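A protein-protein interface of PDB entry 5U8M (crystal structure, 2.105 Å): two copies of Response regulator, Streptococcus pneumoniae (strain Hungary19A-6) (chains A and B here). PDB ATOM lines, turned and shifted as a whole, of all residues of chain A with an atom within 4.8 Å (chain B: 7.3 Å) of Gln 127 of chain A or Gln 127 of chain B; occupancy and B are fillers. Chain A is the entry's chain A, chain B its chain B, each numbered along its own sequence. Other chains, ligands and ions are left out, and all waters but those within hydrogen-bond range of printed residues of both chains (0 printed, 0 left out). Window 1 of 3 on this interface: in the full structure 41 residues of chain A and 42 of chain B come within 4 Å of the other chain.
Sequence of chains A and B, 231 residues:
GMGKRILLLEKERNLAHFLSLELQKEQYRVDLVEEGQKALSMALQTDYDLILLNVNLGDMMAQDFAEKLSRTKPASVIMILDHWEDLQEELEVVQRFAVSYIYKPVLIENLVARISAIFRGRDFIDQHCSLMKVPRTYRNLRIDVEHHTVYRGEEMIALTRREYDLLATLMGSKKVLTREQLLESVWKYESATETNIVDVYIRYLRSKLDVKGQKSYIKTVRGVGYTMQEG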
ATOM      1  N   ASP A 123      20.006   3.751 -22.580  1.00  0.00           N
ATOM      2  CA  ASP A 123      21.180   3.676 -21.730  1.00  0.00           C
ATOM      3  C   ASP A 123      20.817   3.180 -20.331  1.00  0.00           C
ATOM      4  O   ASP A 123      21.640   2.531 -19.682  1.00  0.00           O
ATOM      5  CB  ASP A 123      21.878   5.036 -21.630  1.00  0.00           C
ATOM      6  CG  ASP A 123      22.677   5.369 -22.870  1.00  0.00           C
ATOM      7  OD1 ASP A 123      22.806   4.490 -23.747  1.00  0.00           O
ATOM      8  OD2 ASP A 123      23.179   6.497 -22.969  1.00  0.00           O
ATOM      9  N   PHE A 124      19.602   3.475 -19.860  1.00  0.00           N
ATOM     10  CA  PHE A 124      19.198   3.012 -18.543  1.00  0.00           C
ATOM     11  C   PHE A 124      19.090   1.496 -18.537  1.00  0.00           C
ATOM     12  O   PHE A 124      19.588   0.822 -17.626  1.00  0.00           O
ATOM     13  CB  PHE A 124      17.868   3.658 -18.163  1.00  0.00           C
ATOM     14  CG  PHE A 124      17.515   3.526 -16.701  1.00  0.00           C
ATOM     15  CD1 PHE A 124      18.264   4.182 -15.718  1.00  0.00           C
ATOM     16  CD2 PHE A 124      16.423   2.778 -16.320  1.00  0.00           C
ATOM     17  CE1 PHE A 124      17.919   4.073 -14.374  1.00  0.00           C
ATOM     18  CE2 PHE A 124      16.073   2.654 -14.988  1.00  0.00           C
ATOM     19  CZ  PHE A 124      16.825   3.294 -14.009  1.00  0.00           C
ATOM     20  N   ILE A 125      18.479   0.948 -19.581  1.00  0.00           N
ATOM     21  CA  ILE A 125      18.407  -0.489 -19.743  1.00  0.00           C
ATOM     22  C   ILE A 125      19.793  -1.067 -19.942  1.00  0.00           C
ATOM     23  O   ILE A 125      20.187  -2.019 -19.254  1.00  0.00           O
ATOM     24  CB  ILE A 125      17.465  -0.811 -20.902  1.00  0.00           C
ATOM     25  CG1 ILE A 125      16.060  -0.432 -20.471  1.00  0.00           C
ATOM     26  CG2 ILE A 125      17.544  -2.264 -21.276  1.00  0.00           C
ATOM     27  CD1 ILE A 125      15.114  -0.485 -21.538  1.00  0.00           C
ATOM     28  N   ASP A 126      20.588  -0.443 -20.817  1.00  0.00           N
ATOM     29  CA  ASP A 126      21.850  -1.027 -21.225  1.00  0.00           C
ATOM     30  C   ASP A 126      22.894  -1.007 -20.114  1.00  0.00           C
ATOM     31  O   ASP A 126      23.839  -1.808 -20.153  1.00  0.00           O
ATOM     32  CB  ASP A 126      22.419  -0.300 -22.446  1.00  0.00           C
ATOM     33  CG  ASP A 126      21.756  -0.708 -23.762  1.00  0.00           C
ATOM     34  OD1 ASP A 126      21.062  -1.748 -23.821  1.00  0.00           O
ATOM     35  OD2 ASP A 126      21.967   0.016 -24.762  1.00  0.00           O
ATOM     36  N   GLN A 127      22.766  -0.100 -19.151  1.00  0.00           N
ATOM     37  CA  GLN A 127      23.665  -0.049 -18.008  1.00  0.00           C
ATOM     38  C   GLN A 127      23.151  -0.875 -16.834  1.00  0.00           C
ATOM     39  O   GLN A 127      23.798  -0.885 -15.790  1.00  0.00           O
ATOM     40  CB  GLN A 127      23.887   1.404 -17.566  1.00  0.00           C
ATOM     41  CG  GLN A 127      24.730   2.196 -18.530  1.00  0.00           C
ATOM     42  CD  GLN A 127      24.671   3.678 -18.277  1.00  0.00           C
ATOM     43  OE1 GLN A 127      23.613   4.227 -17.939  1.00  0.00           O
ATOM     44  NE2 GLN A 127      25.807   4.350 -18.456  1.00  0.00           N
ATOM     45  N   HIS A 128      22.002  -1.544 -16.998  1.00  0.00           N
ATOM     46  CA  HIS A 128      21.403  -2.465 -16.009  1.00  0.00           C
ATOM     47  C   HIS A 128      21.087  -1.764 -14.691  1.00  0.00           C
ATOM     48  O   HIS A 128      21.215  -2.341 -13.602  1.00  0.00           O
ATOM     49  CB  HIS A 128      22.294  -3.688 -15.789  1.00  0.00           C
ATOM     50  CG  HIS A 128      22.836  -4.240 -17.065  1.00  0.00           C
ATOM     51  ND1 HIS A 128      22.027  -4.824 -18.019  1.00  0.00           N
ATOM     52  CD2 HIS A 128      24.088  -4.226 -17.582  1.00  0.00           C
ATOM     53  CE1 HIS A 128      22.769  -5.178 -19.053  1.00  0.00           C
ATOM     54  NE2 HIS A 128      24.020  -4.825 -18.815  1.00  0.00           N
ATOM     55  N   CYS A 129      20.631  -0.519 -14.797  1.00  0.00           N
ATOM     56  CA  CYS A 129      20.290   0.253 -13.617  1.00  0.00           C
ATOM     57  C   CYS A 129      19.109  -0.383 -12.906  1.00  0.00           C
ATOM     58  O   CYS A 129      18.130  -0.783 -13.536  1.00  0.00           O
ATOM     59  CB  CYS A 129      19.960   1.689 -14.011  1.00  0.00           C
ATOM     60  SG  CYS A 129      21.248   2.436 -15.102  1.00  0.00           S
ATOM     61  N   TYR A 189      35.313   6.101 -15.746  1.00  0.00           N
ATOM     62  CA  TYR A 189      35.880   6.815 -16.880  1.00  0.00           C
ATOM     63  C   TYR A 189      37.203   7.487 -16.549  1.00  0.00           C
ATOM     64  O   TYR A 189      37.852   8.002 -17.463  1.00  0.00           O
ATOM     65  CB  TYR A 189      34.935   7.889 -17.450  1.00  0.00           C
ATOM     66  CG  TYR A 189      33.566   7.396 -17.835  1.00  0.00           C
ATOM     67  CD1 TYR A 189      33.390   6.528 -18.901  1.00  0.00           C
ATOM     68  CD2 TYR A 189      32.447   7.817 -17.150  1.00  0.00           C
ATOM     69  CE1 TYR A 189      32.134   6.085 -19.261  1.00  0.00           C
ATOM     70  CE2 TYR A 189      31.188   7.377 -17.499  1.00  0.00           C
ATOM     71  CZ  TYR A 189      31.032   6.512 -18.556  1.00  0.00           C
ATOM     72  OH  TYR A 189      29.764   6.080 -18.895  1.00  0.00           O
ATOM     73  N   ARG B 120      31.813  12.998 -17.896  1.00  0.00           N
ATOM     74  CA  ARG B 120      31.077  11.750 -18.072  1.00  0.00           C
ATOM     75  C   ARG B 120      30.777  11.119 -16.714  1.00  0.00           C
ATOM     76  O   ARG B 120      29.643  10.707 -16.448  1.00  0.00           O
ATOM     77  CB  ARG B 120      31.862  10.781 -18.965  1.00  0.00           C
ATOM     78  CG  ARG B 120      31.905  11.147 -20.460  1.00  0.00           C
ATOM     79  CD  ARG B 120      32.279   9.951 -21.352  1.00  0.00           C
ATOM     80  NE  ARG B 120      33.558   9.337 -20.999  1.00  0.00           N
ATOM     81  CZ  ARG B 120      34.753   9.879 -21.238  1.00  0.00           C
ATOM     82  NH1 ARG B 120      34.852  11.066 -21.825  1.00  0.00           N
ATOM     83  NH2 ARG B 120      35.860   9.238 -20.879  1.00  0.00           N
ATOM     84  N   GLY B 121      31.781  11.072 -15.825  1.00  0.00           N
ATOM     85  CA  GLY B 121      31.581  10.504 -14.499  1.00  0.00           C
ATOM     86  C   GLY B 121      30.519  11.226 -13.686  1.00  0.00           C
ATOM     87  O   GLY B 121      29.725  10.596 -12.970  1.00  0.00           O
ATOM     88  N   ARG B 122      30.483  12.558 -13.775  1.00  0.00           N
ATOM     89  CA  ARG B 122      29.444  13.290 -13.062  1.00  0.00           C
ATOM     90  C   ARG B 122      28.084  12.970 -13.656  1.00  0.00           C
ATOM     91  O   ARG B 122      27.107  12.771 -12.921  1.00  0.00           O
ATOM     92  CB  ARG B 122      29.698  14.807 -13.093  1.00  0.00           C
ATOM     93  CG  ARG B 122      30.469  15.342 -11.875  1.00  0.00           C
ATOM     94  CD  ARG B 122      31.822  14.693 -11.750  1.00  0.00           C
ATOM     95  NE  ARG B 122      31.760  13.525 -10.874  1.00  0.00           N
ATOM     96  CZ  ARG B 122      32.449  12.400 -11.036  1.00  0.00           C
ATOM     97  NH1 ARG B 122      32.288  11.411 -10.162  1.00  0.00           N
ATOM     98  NH2 ARG B 122      33.287  12.242 -12.058  1.00  0.00           N
ATOM     99  N   ASP B 123      28.005  12.902 -14.987  1.00  0.00           N
ATOM    100  CA  ASP B 123      26.725  12.647 -15.629  1.00  0.00           C
ATOM    101  C   ASP B 123      26.231  11.250 -15.273  1.00  0.00           C
ATOM    102  O   ASP B 123      25.024  11.033 -15.106  1.00  0.00           O
ATOM    103  CB  ASP B 123      26.835  12.807 -17.147  1.00  0.00           C
ATOM    104  CG  ASP B 123      26.828  14.277 -17.594  1.00  0.00           C
ATOM    105  OD1 ASP B 123      26.340  15.145 -16.835  1.00  0.00           O
ATOM    106  OD2 ASP B 123      27.285  14.556 -18.723  1.00  0.00           O
ATOM    107  N   PHE B 124      27.155  10.294 -15.140  1.00  0.00           N
ATOM    108  CA  PHE B 124      26.758   8.943 -14.766  1.00  0.00           C
ATOM    109  C   PHE B 124      26.181   8.925 -13.355  1.00  0.00           C
ATOM    110  O   PHE B 124      25.133   8.319 -13.118  1.00  0.00           O
ATOM    111  CB  PHE B 124      27.921   7.962 -14.872  1.00  0.00           C
ATOM    112  CG  PHE B 124      27.606   6.595 -14.273  1.00  0.00           C
ATOM    113  CD1 PHE B 124      26.779   5.705 -14.947  1.00  0.00           C
ATOM    114  CD2 PHE B 124      28.104   6.234 -13.029  1.00  0.00           C
ATOM    115  CE1 PHE B 124      26.464   4.463 -14.393  1.00  0.00           C
ATOM    116  CE2 PHE B 124      27.802   4.986 -12.460  1.00  0.00           C
ATOM    117  CZ  PHE B 124      26.984   4.102 -13.145  1.00  0.00           C
ATOM    118  N   ILE B 125      26.840   9.586 -12.399  1.00  0.00           N
ATOM    119  CA  ILE B 125      26.282   9.631 -11.049  1.00  0.00           C
ATOM    120  C   ILE B 125      24.892  10.257 -11.071  1.00  0.00           C
ATOM    121  O   ILE B 125      23.963   9.777 -10.396  1.00  0.00           O
ATOM    122  CB  ILE B 125      27.235  10.388 -10.107  1.00  0.00           C
ATOM    123  CG1 ILE B 125      28.488   9.562  -9.853  1.00  0.00           C
ATOM    124  CG2 ILE B 125      26.563  10.753  -8.816  1.00  0.00           C
ATOM    125  CD1 ILE B 125      28.211   8.187  -9.139  1.00  0.00           C
ATOM    126  N   ASP B 126      24.720  11.323 -11.873  1.00  0.00           N
ATOM    127  CA  ASP B 126      23.454  12.036 -11.969  1.00  0.00           C
ATOM    128  C   ASP B 126      22.320  11.195 -12.568  1.00  0.00           C
ATOM    129  O   ASP B 126      21.165  11.601 -12.448  1.00  0.00           O
ATOM    130  CB  ASP B 126      23.620  13.330 -12.803  1.00  0.00           C
ATOM    131  CG  ASP B 126      24.459  14.417 -12.083  1.00  0.00           C
ATOM    132  OD1 ASP B 126      24.664  14.314 -10.855  1.00  0.00           O
ATOM    133  OD2 ASP B 126      24.904  15.394 -12.740  1.00  0.00           O
ATOM    134  N   GLN B 127      22.572  10.034 -13.181  1.00  0.00           N
ATOM    135  CA  GLN B 127      21.403   9.265 -13.596  1.00  0.00           C
ATOM    136  C   GLN B 127      20.914   8.290 -12.524  1.00  0.00           C
ATOM    137  O   GLN B 127      19.899   7.618 -12.738  1.00  0.00           O
ATOM    138  CB  GLN B 127      21.651   8.548 -14.925  1.00  0.00           C
ATOM    139  CG  GLN B 127      22.767   7.602 -15.012  1.00  0.00           C
ATOM    140  CD  GLN B 127      22.808   6.967 -16.391  1.00  0.00           C
ATOM    141  OE1 GLN B 127      21.822   6.383 -16.859  1.00  0.00           O
ATOM    142  NE2 GLN B 127      23.927   7.107 -17.059  1.00  0.00           N
ATOM    143  N   HIS B 128      21.563   8.249 -11.357  1.00  0.00           N
ATOM    144  CA  HIS B 128      21.097   7.434 -10.229  1.00  0.00           C
ATOM    145  C   HIS B 128      20.938   5.989 -10.671  1.00  0.00           C
ATOM    146  O   HIS B 128      19.893   5.364 -10.498  1.00  0.00           O
ATOM    147  CB  HIS B 128      19.799   7.999  -9.661  1.00  0.00           C
ATOM    148  CG  HIS B 128      19.810   9.492  -9.555  1.00  0.00           C
ATOM    149  ND1 HIS B 128      18.873  10.298 -10.175  1.00  0.00           N
ATOM    150  CD2 HIS B 128      20.652  10.327  -8.901  1.00  0.00           C
ATOM    151  CE1 HIS B 128      19.142  11.565  -9.912  1.00  0.00           C
ATOM    152  NE2 HIS B 128      20.221  11.612  -9.147  1.00  0.00           N
ATOM    153  N   CYS B 129      22.006   5.480 -11.261  1.00  0.00           N
ATOM    154  CA  CYS B 129      22.059   4.151 -11.857  1.00  0.00           C
ATOM    155  C   CYS B 129      22.745   3.219 -10.872  1.00  0.00           C
ATOM    156  O   CYS B 129      23.977   3.184 -10.772  1.00  0.00           O
ATOM    157  CB  CYS B 129      22.808   4.187 -13.183  1.00  0.00           C
ATOM    158  SG  CYS B 129      22.934   2.573 -13.952  1.00  0.00           S
ATOM    159  N   SER B 130      21.945   2.488 -10.120  1.00  0.00           N
ATOM    160  CA  SER B 130      22.472   1.494  -9.205  1.00  0.00           C
ATOM    161  C   SER B 130      22.647   0.202  -9.993  1.00  0.00           C
ATOM    162  O   SER B 130      21.665  -0.449 -10.367  1.00  0.00           O
ATOM    163  CB  SER B 130      21.551   1.307  -8.003  1.00  0.00           C
ATOM    164  OG  SER B 130      22.153   0.396  -7.105  1.00  0.00           O
ATOM    165  N   LEU B 131      23.897  -0.122 -10.299  1.00  0.00           N
ATOM    166  CA  LEU B 131      24.208  -1.303 -11.081  1.00  0.00           C
ATOM    167  C   LEU B 131      23.619  -2.528 -10.392  1.00  0.00           C
ATOM    168  O   LEU B 131      23.750  -2.698  -9.177  1.00  0.00           O
ATOM    169  CB  LEU B 131      25.727  -1.417 -11.224  1.00  0.00           C
ATOM    170  CG  LEU B 131      26.346  -2.285 -12.318  1.00  0.00           C
ATOM    171  CD1 LEU B 131      25.890  -1.835 -13.691  1.00  0.00           C
ATOM    172  CD2 LEU B 131      27.870  -2.227 -12.221  1.00  0.00           C
ATOM    173  N   MET B 132      22.929  -3.360 -11.152  1.00  0.00           N
ATOM    174  CA  MET B 132      22.436  -4.619 -10.614  1.00  0.00           C
ATOM    175  C   MET B 132      22.824  -5.752 -11.562  1.00  0.00           C
ATOM    176  O   MET B 132      23.110  -5.531 -12.745  1.00  0.00           O
ATOM    177  CB  MET B 132      20.927  -4.560 -10.369  1.00  0.00           C
ATOM    178  CG  MET B 132      20.072  -4.667 -11.589  1.00  0.00           C
ATOM    179  SD  MET B 132      18.335  -4.781 -11.115  1.00  0.00           S
ATOM    180  CE  MET B 132      17.634  -5.344 -12.672  1.00  0.00           C
ATOM    181  N   ARG B 161      13.887  -3.639 -30.410  1.00  0.00           N
ATOM    182  CA  ARG B 161      14.477  -2.989 -29.246  1.00  0.00           C
ATOM    183  C   ARG B 161      13.486  -2.897 -28.099  1.00  0.00           C
ATOM    184  O   ARG B 161      13.802  -3.260 -26.959  1.00  0.00           O
ATOM    185  CB  ARG B 161      14.972  -1.582 -29.599  1.00  0.00           C
ATOM    186  CG  ARG B 161      15.615  -0.868 -28.404  1.00  0.00           C
ATOM    187  CD  ARG B 161      16.942  -1.523 -28.079  1.00  0.00           C
ATOM    188  NE  ARG B 161      17.214  -1.558 -26.650  1.00  0.00           N
ATOM    189  CZ  ARG B 161      18.392  -1.322 -26.087  1.00  0.00           C
ATOM    190  NH1 ARG B 161      19.455  -0.989 -26.811  1.00  0.00           N
ATOM    191  NH2 ARG B 161      18.490  -1.391 -24.776  1.00  0.00           N
ATOM    192  N   LYS B 188      10.992   4.938 -20.123  1.00  0.00           N
ATOM    193  CA  LYS B 188      11.554   5.930 -19.218  1.00  0.00           C
ATOM    194  C   LYS B 188      12.019   7.140 -20.013  1.00  0.00           C
ATOM    195  O   LYS B 188      12.590   7.010 -21.102  1.00  0.00           O
ATOM    196  CB  LYS B 188      12.730   5.334 -18.428  1.00  0.00           C
ATOM    197  CG  LYS B 188      13.066   6.039 -17.141  1.00  0.00           C
ATOM    198  CD  LYS B 188      14.358   5.471 -16.559  1.00  0.00           C
ATOM    199  CE  LYS B 188      14.371   5.498 -15.040  1.00  0.00           C
ATOM    200  NZ  LYS B 188      13.959   6.806 -14.493  1.00  0.00           N
ATOM    201  N   TYR B 189      11.740   8.316 -19.468  1.00  0.00           N
ATOM    202  CA  TYR B 189      12.156   9.608 -19.972  1.00  0.00           C
ATOM    203  C   TYR B 189      11.275  10.086 -21.121  1.00  0.00           C
ATOM    204  O   TYR B 189      11.495  11.209 -21.594  1.00  0.00           O
ATOM    205  CB  TYR B 189      13.616   9.627 -20.446  1.00  0.00           C
ATOM    206  CG  TYR B 189      14.645   9.200 -19.418  1.00  0.00           C
ATOM    207  CD1 TYR B 189      14.979  10.013 -18.346  1.00  0.00           C
ATOM    208  CD2 TYR B 189      15.299   7.993 -19.535  1.00  0.00           C
ATOM    209  CE1 TYR B 189      15.935   9.616 -17.406  1.00  0.00           C
ATOM    210  CE2 TYR B 189      16.249   7.593 -18.612  1.00  0.00           C
ATOM    211  CZ  TYR B 189      16.564   8.400 -17.549  1.00  0.00           C
ATOM    212  OH  TYR B 189      17.522   7.979 -16.647  1.00  0.00           O
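Of the 16 printed residues of chain B, 11 touch a printed residue of chain A.
Printed residues of chain A that touch a printed residue of chain B: Phe 124, Ile 125, Asp 126, Gln 127, His 128, Cys 129 and Tyr 189.
Hydrophobic or aromatic side chains of chain A within 4 Å of the printed part of chain B: Phe 124, Ile 125, His 128 and Tyr 189.
Among the printed residues, 14 pairs touch across the chains.
Among the printed residues, Asp or Glu carboxylates within 4 Å of a Lys or Arg side-chain nitrogen of the other chain: Asp 126 of chain A with Arg 161 of chain B (2.8 Å).
Phe 124 of chain A touches Tyr 189 of chain B, but with the chains exchanged Tyr 189 of chain A does not touch Phe 124 of chain B (4.2 Å).
Gln 127 of chain A touches Phe 124 of chain B, but with the chains exchanged Phe 124 of chain A does not touch Gln 127 of chain B (4.3 Å).
Gln 127 of chain B touches its own counterpart, Gln 127 of chain A.
Cys 129 of chain B touches its own counterpart, Cys 129 of chain A.
Of chain A, only Gln 127 comes within 4 Å of Gln 127 of chain B.
Of the printed residues of chain A, Phe 124 of chain B touches Gln 127 (3.9 Å).
Printed residues of chain A within 4 Å of Gly 121 of chain B: Tyr 189.
Of the printed residues of chain B, Cys 129 of chain A touches Cys 129 and Ser 130.
Printed residues of chain A within 4 Å of Arg 161 of chain B: Ile 125 and Asp 126.
Of the printed residues of chain B, His 128 of chain A touches Ser 130 and Met 132.
The nearest residue of chain B that does not touch Gln 127 of chain A is Met 132 of chain B (5.3 Å).
The nearest printed residue of chain A that does not touch Gln 127 of chain B is Phe 124 of chain A (4.3 Å).
Among the printed residues, merely in contact across the chains: Gln 127 of chain A with Leu 131 of chain B, Phe 124 of chain A with Lys 188 of chain B, Tyr 189 of chain A with Arg 120 of chain B, Tyr 189 of chain A with Gly 121 of chain B, Cys 129 of chain A with Ser 130 of chain B, Ile 125 of chain A with Arg 161 of chain B, His 128 of chain A with Ser 130 of chain B, Gln 127 of chain A with Phe 124 of chain B, Gln 127 of chain A with Cys 129 of chain B and Phe 124 of chain A with Tyr 189 of chain B.
OE1 of Gln 127 of chain A sits close to O of Asp 123 of chain A, at 3.1 Å.
The backbone carbonyl oxygen of Phe 124 of chain A lies within hydrogen-bond range of the backbone NH of Cys 129 of chain A, at 3.3 Å.
The backbone carbonyl oxygen (O) of Asp 126 of chain A lies within hydrogen-bond range of a ring nitrogen (NE2) of His 128 of chain A (3.3 Å).
The guanidinium group (NH2) of Arg 161 of chain B lies within salt-bridge range of the side-chain carboxylate (OD1) of Asp 126 of chain A.
The side-chain amide oxygen (OE1) of Gln 127 of chain A sits close to the side-chain amide oxygen (OE1) of Gln 127 of chain B, at 3.0 Å.
The backbone carbonyl oxygen of His 128 of chain A sits at hydrogen-bond distance from the backbone NH of Met 132 of chain B (3.2 Å).
SG of Cys 129 of chain B forms a disulfide with SG of Cys 129 of chain A, 2.0 Å away.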
